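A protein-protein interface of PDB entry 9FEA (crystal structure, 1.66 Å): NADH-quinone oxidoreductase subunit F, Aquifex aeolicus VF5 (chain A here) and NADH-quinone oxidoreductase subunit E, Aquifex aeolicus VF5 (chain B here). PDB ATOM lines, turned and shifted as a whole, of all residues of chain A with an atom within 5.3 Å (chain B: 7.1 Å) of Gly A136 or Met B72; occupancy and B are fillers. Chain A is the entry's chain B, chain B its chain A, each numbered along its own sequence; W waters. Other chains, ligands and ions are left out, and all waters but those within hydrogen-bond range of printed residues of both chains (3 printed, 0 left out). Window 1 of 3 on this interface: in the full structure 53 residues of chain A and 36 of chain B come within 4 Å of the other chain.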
ATOM      1  N   ILE A 134     -15.315 -18.815 -34.427  1.00  0.00           N
ATOM      2  CA  ILE A 134     -14.334 -19.889 -34.504  1.00  0.00           C
ATOM      3  C   ILE A 134     -14.378 -20.729 -33.240  1.00  0.00           C
ATOM      4  O   ILE A 134     -14.460 -20.216 -32.129  1.00  0.00           O
ATOM      5  CB  ILE A 134     -12.922 -19.355 -34.776  1.00  0.00           C
ATOM      6  CG1 ILE A 134     -11.941 -20.506 -35.055  1.00  0.00           C
ATOM      7  CG2 ILE A 134     -12.429 -18.429 -33.663  1.00  0.00           C
ATOM      8  CD1 ILE A 134     -10.610 -20.030 -35.584  1.00  0.00           C
ATOM      9  N   ARG A 135     -14.315 -22.059 -33.424  1.00  0.00           N
ATOM     10  CA  ARG A 135     -14.379 -22.937 -32.268  1.00  0.00           C
ATOM     11  C   ARG A 135     -13.280 -22.593 -31.275  1.00  0.00           C
ATOM     12  O   ARG A 135     -12.199 -22.141 -31.637  1.00  0.00           O
ATOM     13  CB  ARG A 135     -14.297 -24.403 -32.704  1.00  0.00           C
ATOM     14  CG  ARG A 135     -12.976 -24.787 -33.346  1.00  0.00           C
ATOM     15  CD  ARG A 135     -12.992 -26.242 -33.761  1.00  0.00           C
ATOM     16  NE  ARG A 135     -13.100 -27.154 -32.617  1.00  0.00           N
ATOM     17  CZ  ARG A 135     -12.947 -28.474 -32.695  1.00  0.00           C
ATOM     18  NH1 ARG A 135     -12.765 -29.041 -33.878  1.00  0.00           N
ATOM     19  NH2 ARG A 135     -12.931 -29.206 -31.589  1.00  0.00           N
ATOM     20  N   GLY A 136     -13.559 -22.839 -29.992  1.00  0.00           N
ATOM     21  CA  GLY A 136     -12.637 -22.522 -28.920  1.00  0.00           C
ATOM     22  C   GLY A 136     -11.365 -23.363 -28.957  1.00  0.00           C
ATOM     23  O   GLY A 136     -10.346 -22.908 -28.465  1.00  0.00           O
ATOM     24  N   GLU A 137     -11.410 -24.555 -29.569  1.00  0.00           N
ATOM     25  CA  GLU A 137     -10.246 -25.432 -29.658  1.00  0.00           C
ATOM     26  C   GLU A 137      -9.345 -25.108 -30.861  1.00  0.00           C
ATOM     27  O   GLU A 137      -8.394 -25.849 -31.116  1.00  0.00           O
ATOM     28  CB  GLU A 137     -10.694 -26.891 -29.761  1.00  0.00           C
ATOM     29  CG  GLU A 137     -11.646 -27.341 -28.652  1.00  0.00           C
ATOM     30  CD  GLU A 137     -13.126 -27.044 -28.873  1.00  0.00           C
ATOM     31  OE1 GLU A 137     -13.480 -26.366 -29.857  1.00  0.00           O
ATOM     32  OE2 GLU A 137     -13.931 -27.539 -28.059  1.00  0.00           O
ATOM     33  N   TYR A 138      -9.610 -23.982 -31.558  1.00  0.00           N
ATOM     34  CA  TYR A 138      -8.712 -23.420 -32.553  1.00  0.00           C
ATOM     35  C   TYR A 138      -8.124 -22.099 -32.041  1.00  0.00           C
ATOM     36  O   TYR A 138      -8.379 -21.042 -32.618  1.00  0.00           O
ATOM     37  CB  TYR A 138      -9.436 -23.182 -33.881  1.00  0.00           C
ATOM     38  CG  TYR A 138      -9.797 -24.370 -34.765  1.00  0.00           C
ATOM     39  CD1 TYR A 138      -9.291 -25.653 -34.549  1.00  0.00           C
ATOM     40  CD2 TYR A 138     -10.619 -24.189 -35.879  1.00  0.00           C
ATOM     41  CE1 TYR A 138      -9.600 -26.707 -35.395  1.00  0.00           C
ATOM     42  CE2 TYR A 138     -10.945 -25.238 -36.726  1.00  0.00           C
ATOM     43  CZ  TYR A 138     -10.431 -26.499 -36.484  1.00  0.00           C
ATOM     44  OH  TYR A 138     -10.708 -27.553 -37.325  1.00  0.00           O
ATOM     45  N   PRO A 139      -7.325 -22.093 -30.953  1.00  0.00           N
ATOM     46  CA  PRO A 139      -6.777 -20.848 -30.426  1.00  0.00           C
ATOM     47  C   PRO A 139      -5.797 -20.177 -31.380  1.00  0.00           C
ATOM     48  O   PRO A 139      -5.803 -18.960 -31.500  1.00  0.00           O
ATOM     49  CB  PRO A 139      -6.143 -21.264 -29.107  1.00  0.00           C
ATOM     50  CG  PRO A 139      -5.784 -22.711 -29.344  1.00  0.00           C
ATOM     51  CD  PRO A 139      -6.940 -23.261 -30.137  1.00  0.00           C
ATOM     52  N   ARG A 175     -15.312 -16.557 -30.139  1.00  0.00           N
ATOM     53  CA  ARG A 175     -14.776 -17.882 -29.896  1.00  0.00           C
ATOM     54  C   ARG A 175     -15.870 -18.760 -29.295  1.00  0.00           C
ATOM     55  O   ARG A 175     -16.606 -18.325 -28.406  1.00  0.00           O
ATOM     56  CB  ARG A 175     -13.618 -17.894 -28.898  1.00  0.00           C
ATOM     57  CG  ARG A 175     -12.393 -17.140 -29.380  1.00  0.00           C
ATOM     58  CD  ARG A 175     -11.208 -17.279 -28.461  1.00  0.00           C
ATOM     59  NE  ARG A 175     -10.666 -18.639 -28.441  1.00  0.00           N
ATOM     60  CZ  ARG A 175      -9.881 -19.095 -27.478  1.00  0.00           C
ATOM     61  NH1 ARG A 175      -9.533 -18.297 -26.483  1.00  0.00           N
ATOM     62  NH2 ARG A 175      -9.446 -20.349 -27.495  1.00  0.00           N
ATOM     63  N   GLY A 176     -15.918 -20.011 -29.755  1.00  0.00           N
ATOM     64  CA  GLY A 176     -16.758 -21.022 -29.145  1.00  0.00           C
ATOM     65  C   GLY A 176     -16.121 -21.507 -27.851  1.00  0.00           C
ATOM     66  O   GLY A 176     -15.054 -21.015 -27.477  1.00  0.00           O
ATOM     67  N   ALA A 177     -16.767 -22.475 -27.189  1.00  0.00           N
ATOM     68  CA  ALA A 177     -16.245 -22.967 -25.919  1.00  0.00           C
ATOM     69  C   ALA A 177     -16.635 -24.427 -25.669  1.00  0.00           C
ATOM     70  O   ALA A 177     -16.833 -24.827 -24.519  1.00  0.00           O
ATOM     71  CB  ALA A 177     -16.697 -22.051 -24.817  1.00  0.00           C
ATOM     72  N   GLY A 178     -16.711 -25.217 -26.750  1.00  0.00           N
ATOM     73  CA  GLY A 178     -16.684 -26.666 -26.643  1.00  0.00           C
ATOM     74  C   GLY A 178     -17.908 -27.384 -27.213  1.00  0.00           C
ATOM     75  O   GLY A 178     -18.034 -28.607 -27.047  1.00  0.00           O
ATOM     76  N   HIS B  35     -13.140 -17.608 -21.052  1.00  0.00           N
ATOM     77  CA  HIS B  35     -11.849 -18.102 -21.500  1.00  0.00           C
ATOM     78  C   HIS B  35     -10.744 -17.374 -20.739  1.00  0.00           C
ATOM     79  O   HIS B  35      -9.804 -17.990 -20.247  1.00  0.00           O
ATOM     80  CB  HIS B  35     -11.694 -17.954 -23.028  1.00  0.00           C
ATOM     81  CG  HIS B  35     -12.336 -19.026 -23.858  1.00  0.00           C
ATOM     82  ND1 HIS B  35     -12.002 -20.360 -23.771  1.00  0.00           N
ATOM     83  CD2 HIS B  35     -13.246 -18.938 -24.855  1.00  0.00           C
ATOM     84  CE1 HIS B  35     -12.713 -21.046 -24.666  1.00  0.00           C
ATOM     85  NE2 HIS B  35     -13.474 -20.201 -25.342  1.00  0.00           N
ATOM     86  N   GLN B  38     -10.546 -18.517 -17.146  1.00  0.00           N
ATOM     87  CA  GLN B  38     -10.021 -19.854 -16.975  1.00  0.00           C
ATOM     88  C   GLN B  38      -8.509 -19.855 -17.210  1.00  0.00           C
ATOM     89  O   GLN B  38      -7.770 -20.571 -16.533  1.00  0.00           O
ATOM     90  CB  GLN B  38     -10.750 -20.849 -17.875  1.00  0.00           C
ATOM     91  CG  GLN B  38     -10.179 -22.252 -17.732  1.00  0.00           C
ATOM     92  CD  GLN B  38     -11.208 -23.320 -17.995  1.00  0.00           C
ATOM     93  OE1 GLN B  38     -12.178 -23.457 -17.246  1.00  0.00           O
ATOM     94  NE2 GLN B  38     -11.013 -24.059 -19.077  1.00  0.00           N
ATOM     95  N   ILE B  44     -12.576 -22.116 -13.704  1.00  0.00           N
ATOM     96  CA  ILE B  44     -13.509 -21.021 -13.462  1.00  0.00           C
ATOM     97  C   ILE B  44     -13.857 -21.019 -11.977  1.00  0.00           C
ATOM     98  O   ILE B  44     -14.635 -21.860 -11.532  1.00  0.00           O
ATOM     99  CB  ILE B  44     -14.794 -21.140 -14.309  1.00  0.00           C
ATOM    100  CG1 ILE B  44     -14.526 -21.170 -15.815  1.00  0.00           C
ATOM    101  CG2 ILE B  44     -15.784 -20.033 -13.926  1.00  0.00           C
ATOM    102  CD1 ILE B  44     -13.971 -19.877 -16.374  1.00  0.00           C
ATOM    103  N   VAL B  67     -21.743 -21.283 -18.302  1.00  0.00           N
ATOM    104  CA  VAL B  67     -20.571 -22.038 -17.867  1.00  0.00           C
ATOM    105  C   VAL B  67     -20.871 -23.541 -17.919  1.00  0.00           C
ATOM    106  O   VAL B  67     -20.026 -24.318 -18.366  1.00  0.00           O
ATOM    107  CB  VAL B  67     -20.052 -21.624 -16.477  1.00  0.00           C
ATOM    108  CG1 VAL B  67     -18.923 -22.522 -15.989  1.00  0.00           C
ATOM    109  CG2 VAL B  67     -19.563 -20.185 -16.460  1.00  0.00           C
ATOM    110  N   PHE B  69     -23.013 -25.141 -19.771  1.00  0.00           N
ATOM    111  CA  PHE B  69     -23.326 -25.607 -21.114  1.00  0.00           C
ATOM    112  C   PHE B  69     -22.064 -25.889 -21.930  1.00  0.00           C
ATOM    113  O   PHE B  69     -22.055 -26.853 -22.705  1.00  0.00           O
ATOM    114  CB  PHE B  69     -24.130 -24.562 -21.889  1.00  0.00           C
ATOM    115  CG  PHE B  69     -24.533 -25.019 -23.281  1.00  0.00           C
ATOM    116  CD1 PHE B  69     -25.669 -25.800 -23.461  1.00  0.00           C
ATOM    117  CD2 PHE B  69     -23.766 -24.683 -24.388  1.00  0.00           C
ATOM    118  CE1 PHE B  69     -26.038 -26.217 -24.727  1.00  0.00           C
ATOM    119  CE2 PHE B  69     -24.143 -25.097 -25.652  1.00  0.00           C
ATOM    120  CZ  PHE B  69     -25.273 -25.869 -25.815  1.00  0.00           C
ATOM    121  N   TYR B  70     -21.037 -25.042 -21.787  1.00  0.00           N
ATOM    122  CA  TYR B  70     -19.874 -25.080 -22.675  1.00  0.00           C
ATOM    123  C   TYR B  70     -18.757 -25.929 -22.065  1.00  0.00           C
ATOM    124  O   TYR B  70     -18.238 -25.622 -20.994  1.00  0.00           O
ATOM    125  CB  TYR B  70     -19.412 -23.662 -22.994  1.00  0.00           C
ATOM    126  CG  TYR B  70     -20.361 -22.913 -23.918  1.00  0.00           C
ATOM    127  CD1 TYR B  70     -20.410 -23.201 -25.272  1.00  0.00           C
ATOM    128  CD2 TYR B  70     -21.229 -21.945 -23.422  1.00  0.00           C
ATOM    129  CE1 TYR B  70     -21.267 -22.516 -26.117  1.00  0.00           C
ATOM    130  CE2 TYR B  70     -22.111 -21.273 -24.251  1.00  0.00           C
ATOM    131  CZ  TYR B  70     -22.108 -21.542 -25.608  1.00  0.00           C
ATOM    132  OH  TYR B  70     -22.962 -20.872 -26.432  1.00  0.00           O
ATOM    133  N   ASP B  71     -18.386 -26.997 -22.777  1.00  0.00           N
ATOM    134  CA  ASP B  71     -17.618 -28.085 -22.198  1.00  0.00           C
ATOM    135  C   ASP B  71     -16.167 -27.695 -21.924  1.00  0.00           C
ATOM    136  O   ASP B  71     -15.499 -28.368 -21.144  1.00  0.00           O
ATOM    137  CB  ASP B  71     -17.632 -29.319 -23.084  1.00  0.00           C
ATOM    138  CG  ASP B  71     -18.869 -30.203 -23.011  1.00  0.00           C
ATOM    139  OD1 ASP B  71     -19.786 -29.906 -22.192  1.00  0.00           O
ATOM    140  OD2 ASP B  71     -18.890 -31.202 -23.765  1.00  0.00           O
ATOM    141  N   MET B  72     -15.670 -26.621 -22.547  1.00  0.00           N
ATOM    142  CA  MET B  72     -14.282 -26.238 -22.330  1.00  0.00           C
ATOM    143  C   MET B  72     -14.074 -25.698 -20.918  1.00  0.00           C
ATOM    144  O   MET B  72     -12.948 -25.729 -20.441  1.00  0.00           O
ATOM    145  CB  MET B  72     -13.809 -25.178 -23.327  1.00  0.00           C
ATOM    146  CG  MET B  72     -13.522 -25.779 -24.689  1.00  0.00           C
ATOM    147  SD  MET B  72     -12.770 -24.617 -25.837  1.00  0.00           S
ATOM    148  CE  MET B  72     -11.095 -24.405 -25.208  1.00  0.00           C
ATOM    149  N   PHE B  73     -15.146 -25.240 -20.258  1.00  0.00           N
ATOM    150  CA  PHE B  73     -15.015 -24.590 -18.961  1.00  0.00           C
ATOM    151  C   PHE B  73     -15.114 -25.622 -17.842  1.00  0.00           C
ATOM    152  O   PHE B  73     -15.931 -26.532 -17.923  1.00  0.00           O
ATOM    153  CB  PHE B  73     -16.076 -23.508 -18.788  1.00  0.00           C
ATOM    154  CG  PHE B  73     -16.021 -22.434 -19.860  1.00  0.00           C
ATOM    155  CD1 PHE B  73     -14.819 -21.819 -20.186  1.00  0.00           C
ATOM    156  CD2 PHE B  73     -17.172 -22.062 -20.551  1.00  0.00           C
ATOM    157  CE1 PHE B  73     -14.768 -20.855 -21.178  1.00  0.00           C
ATOM    158  CE2 PHE B  73     -17.114 -21.083 -21.529  1.00  0.00           C
ATOM    159  CZ  PHE B  73     -15.910 -20.487 -21.832  1.00  0.00           C
ATOM    160  N   ASP B  74     -14.289 -25.430 -16.806  1.00  0.00           N
ATOM    161  CA  ASP B  74     -14.140 -26.357 -15.692  1.00  0.00           C
ATOM    162  C   ASP B  74     -14.233 -25.571 -14.384  1.00  0.00           C
ATOM    163  O   ASP B  74     -13.385 -24.724 -14.115  1.00  0.00           O
ATOM    164  CB  ASP B  74     -12.809 -27.082 -15.827  1.00  0.00           C
ATOM    165  CG  ASP B  74     -12.501 -28.182 -14.826  1.00  0.00           C
ATOM    166  OD1 ASP B  74     -13.309 -28.376 -13.887  1.00  0.00           O
ATOM    167  OD2 ASP B  74     -11.427 -28.833 -14.988  1.00  0.00           O
ATOM    168  N   ARG B  82      -3.820 -27.976 -19.165  1.00  0.00           N
ATOM    169  CA  ARG B  82      -4.810 -28.959 -19.568  1.00  0.00           C
ATOM    170  C   ARG B  82      -4.284 -29.729 -20.770  1.00  0.00           C
ATOM    171  O   ARG B  82      -4.041 -29.133 -21.818  1.00  0.00           O
ATOM    172  CB  ARG B  82      -6.143 -28.267 -19.851  1.00  0.00           C
ATOM    173  CG  ARG B  82      -6.858 -27.809 -18.590  1.00  0.00           C
ATOM    174  CD  ARG B  82      -7.982 -26.800 -18.818  1.00  0.00           C
ATOM    175  NE  ARG B  82      -8.443 -26.313 -17.508  1.00  0.00           N
ATOM    176  CZ  ARG B  82      -9.184 -27.023 -16.692  1.00  0.00           C
ATOM    177  NH1 ARG B  82      -9.255 -26.716 -15.414  1.00  0.00           N
ATOM    178  NH2 ARG B  82      -9.772 -28.116 -17.147  1.00  0.00           N
ATOM    179  N   ARG B  84      -5.541 -31.867 -23.410  1.00  0.00           N
ATOM    180  CA  ARG B  84      -6.772 -32.310 -24.028  1.00  0.00           C
ATOM    181  C   ARG B  84      -6.430 -33.451 -24.976  1.00  0.00           C
ATOM    182  O   ARG B  84      -5.670 -33.247 -25.912  1.00  0.00           O
ATOM    183  CB  ARG B  84      -7.469 -31.157 -24.756  1.00  0.00           C
ATOM    184  CG  ARG B  84      -8.066 -30.136 -23.798  1.00  0.00           C
ATOM    185  CD  ARG B  84      -8.606 -28.924 -24.510  1.00  0.00           C
ATOM    186  NE  ARG B  84      -9.475 -28.151 -23.626  1.00  0.00           N
ATOM    187  CZ  ARG B  84      -9.117 -27.087 -22.912  1.00  0.00           C
ATOM    188  NH1 ARG B  84     -10.033 -26.446 -22.198  1.00  0.00           N
ATOM    189  NH2 ARG B  84      -7.860 -26.671 -22.929  1.00  0.00           N
ATOM    190  N   VAL B 123      -7.841 -34.113 -20.041  1.00  0.00           N
ATOM    191  CA  VAL B 123      -9.211 -33.808 -20.402  1.00  0.00           C
ATOM    192  C   VAL B 123      -9.538 -34.560 -21.684  1.00  0.00           C
ATOM    193  O   VAL B 123      -9.055 -34.204 -22.771  1.00  0.00           O
ATOM    194  CB  VAL B 123      -9.388 -32.290 -20.599  1.00  0.00           C
ATOM    195  CG1 VAL B 123     -10.833 -31.937 -20.960  1.00  0.00           C
ATOM    196  CG2 VAL B 123      -8.929 -31.523 -19.367  1.00  0.00           C
ATOM    197  N   VAL B 125     -11.582 -35.142 -24.877  1.00  0.00           N
ATOM    198  CA  VAL B 125     -12.324 -34.212 -25.717  1.00  0.00           C
ATOM    199  C   VAL B 125     -12.718 -34.889 -27.024  1.00  0.00           C
ATOM    200  O   VAL B 125     -12.104 -35.852 -27.463  1.00  0.00           O
ATOM    201  CB  VAL B 125     -11.581 -32.895 -26.035  1.00  0.00           C
ATOM    202  CG1 VAL B 125     -11.321 -32.096 -24.773  1.00  0.00           C
ATOM    203  CG2 VAL B 125     -10.297 -33.100 -26.828  1.00  0.00           C
ATOM    204  N   MET B 138      -3.701 -31.552 -27.104  1.00  0.00           N
ATOM    205  CA  MET B 138      -3.297 -30.183 -26.870  1.00  0.00           C
ATOM    206  C   MET B 138      -2.704 -30.091 -25.469  1.00  0.00           C
ATOM    207  O   MET B 138      -3.063 -30.871 -24.609  1.00  0.00           O
ATOM    208  CB  MET B 138      -4.475 -29.207 -26.959  1.00  0.00           C
ATOM    209  CG  MET B 138      -5.241 -29.265 -28.252  1.00  0.00           C
ATOM    210  SD  MET B 138      -6.599 -28.073 -28.296  1.00  0.00           S
ATOM    211  CE  MET B 138      -5.641 -26.560 -28.450  1.00  0.00           C
ATOM    212  N   ASP B 141      -2.996 -24.216 -25.198  1.00  0.00           N
ATOM    213  CA  ASP B 141      -3.329 -23.803 -26.561  1.00  0.00           C
ATOM    214  C   ASP B 141      -2.479 -24.529 -27.614  1.00  0.00           C
ATOM    215  O   ASP B 141      -2.768 -24.434 -28.816  1.00  0.00           O
ATOM    216  CB  ASP B 141      -3.206 -22.295 -26.735  1.00  0.00           C
ATOM    217  CG  ASP B 141      -4.313 -21.437 -26.128  1.00  0.00           C
ATOM    218  OD1 ASP B 141      -5.276 -22.008 -25.604  1.00  0.00           O
ATOM    219  OD2 ASP B 141      -4.212 -20.191 -26.217  1.00  0.00           O
HETATM  220  O   HOH W   1      -7.895 -21.412 -25.413  1.00  0.00           O
HETATM  221  O   HOH W   2     -20.395 -27.814 -24.810  1.00  0.00           O
HETATM  222  O   HOH W   3     -20.689 -30.386 -25.848  1.00  0.00           O
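Gly A136 touches Met B72. Glu A137 touches Met B72. Met B138 touches Glu A137. Met B138 touches Pro A139 (CE to CD, 3.9 Å). CG of Asp B141 touches CB of Pro A139, at 3.5 Å. His B35 touches Arg A175. Ala A177 touches His B35. Ala A177 touches Tyr B70 (O to CB, 3.2 Å). Phe B73 touches Ala A177. CG of Met B72 touches CA of Gly A178, at 3.8 Å.
The backbone carbonyl oxygen (O) of Met B72 sits at hydrogen-bond distance from the guanidinium group (NH1) of Arg B84. The backbone carbonyl oxygen of Arg B84 sits at hydrogen-bond distance from the backbone NH of Met B138, 2.9 Å away. O of Ile A134 is in hydrogen-bond range of N of Gly A176, at 2.8 Å. The side-chain carboxylate (OE1) of Glu A137 is in salt-bridge range of the guanidinium group (NE) of Arg A135, 2.9 Å away. NH2 of Arg A175 lies within hydrogen-bond range of O of Gly A136 (2.9 Å). N of Gly A136 lies close to O of Gly A176, 3.4 Å away.
Hydrophobic or aromatic side chains of chain B that line the printed part of chain A: His B35, Tyr B70, Met B72, Phe B73 and Met B138. Of the 10 printed residues of chain A, 7 touch a printed residue of chain B. Hydrophobic or aromatic side chains of chain A that line the printed part of chain B: Pro A139 and Ala A177. Along chain A the printed residues that touch a printed residue of chain B span positions 136 to 178.
The backbone carbonyl oxygen (O) of Gly A176 lies within hydrogen-bond range of a ring nitrogen (NE2) of His B35 (2.8 Å). The backbone NH (N) of Asp B71 is in hydrogen-bond range of the backbone carbonyl oxygen (O) of Ala A177 (3.2 Å). N of Met B72 sits at hydrogen-bond distance from O of Ala A177.
Water W1 bridges the side-chain carboxylate of Asp B141 (2.7 Å) and the guanidinium group of Arg A175 (2.8 Å). Water W2 lies within hydrogen-bond range of O of Phe B69 (2.8 Å), N of Asp B71 (3.0 Å) and O of Gly A178 (3.3 Å). Water W3 lies within hydrogen-bond range of OD2 of Asp B71 and O of Gly A178.
Of chain B, only Met B72 comes within 4 Å of Gly A136. Of the printed residues of chain B, Gly A176 touches His B35. Of the printed residues of chain A, Tyr B70 touches Ala A177 (3.2 Å). Met B72 touches just these residues of chain A: Gly A136 (3.6 Å), Glu A137 (3.8 Å), Ala A177 (2.9 Å) and Gly A178 (3.8 Å). Val B123 touches none of the printed residues of chain A. Val B125 touches none of the printed residues of chain A. The nearest printed residue of chain B that does not touch Ala A177 is Phe B69 (5.9 Å).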
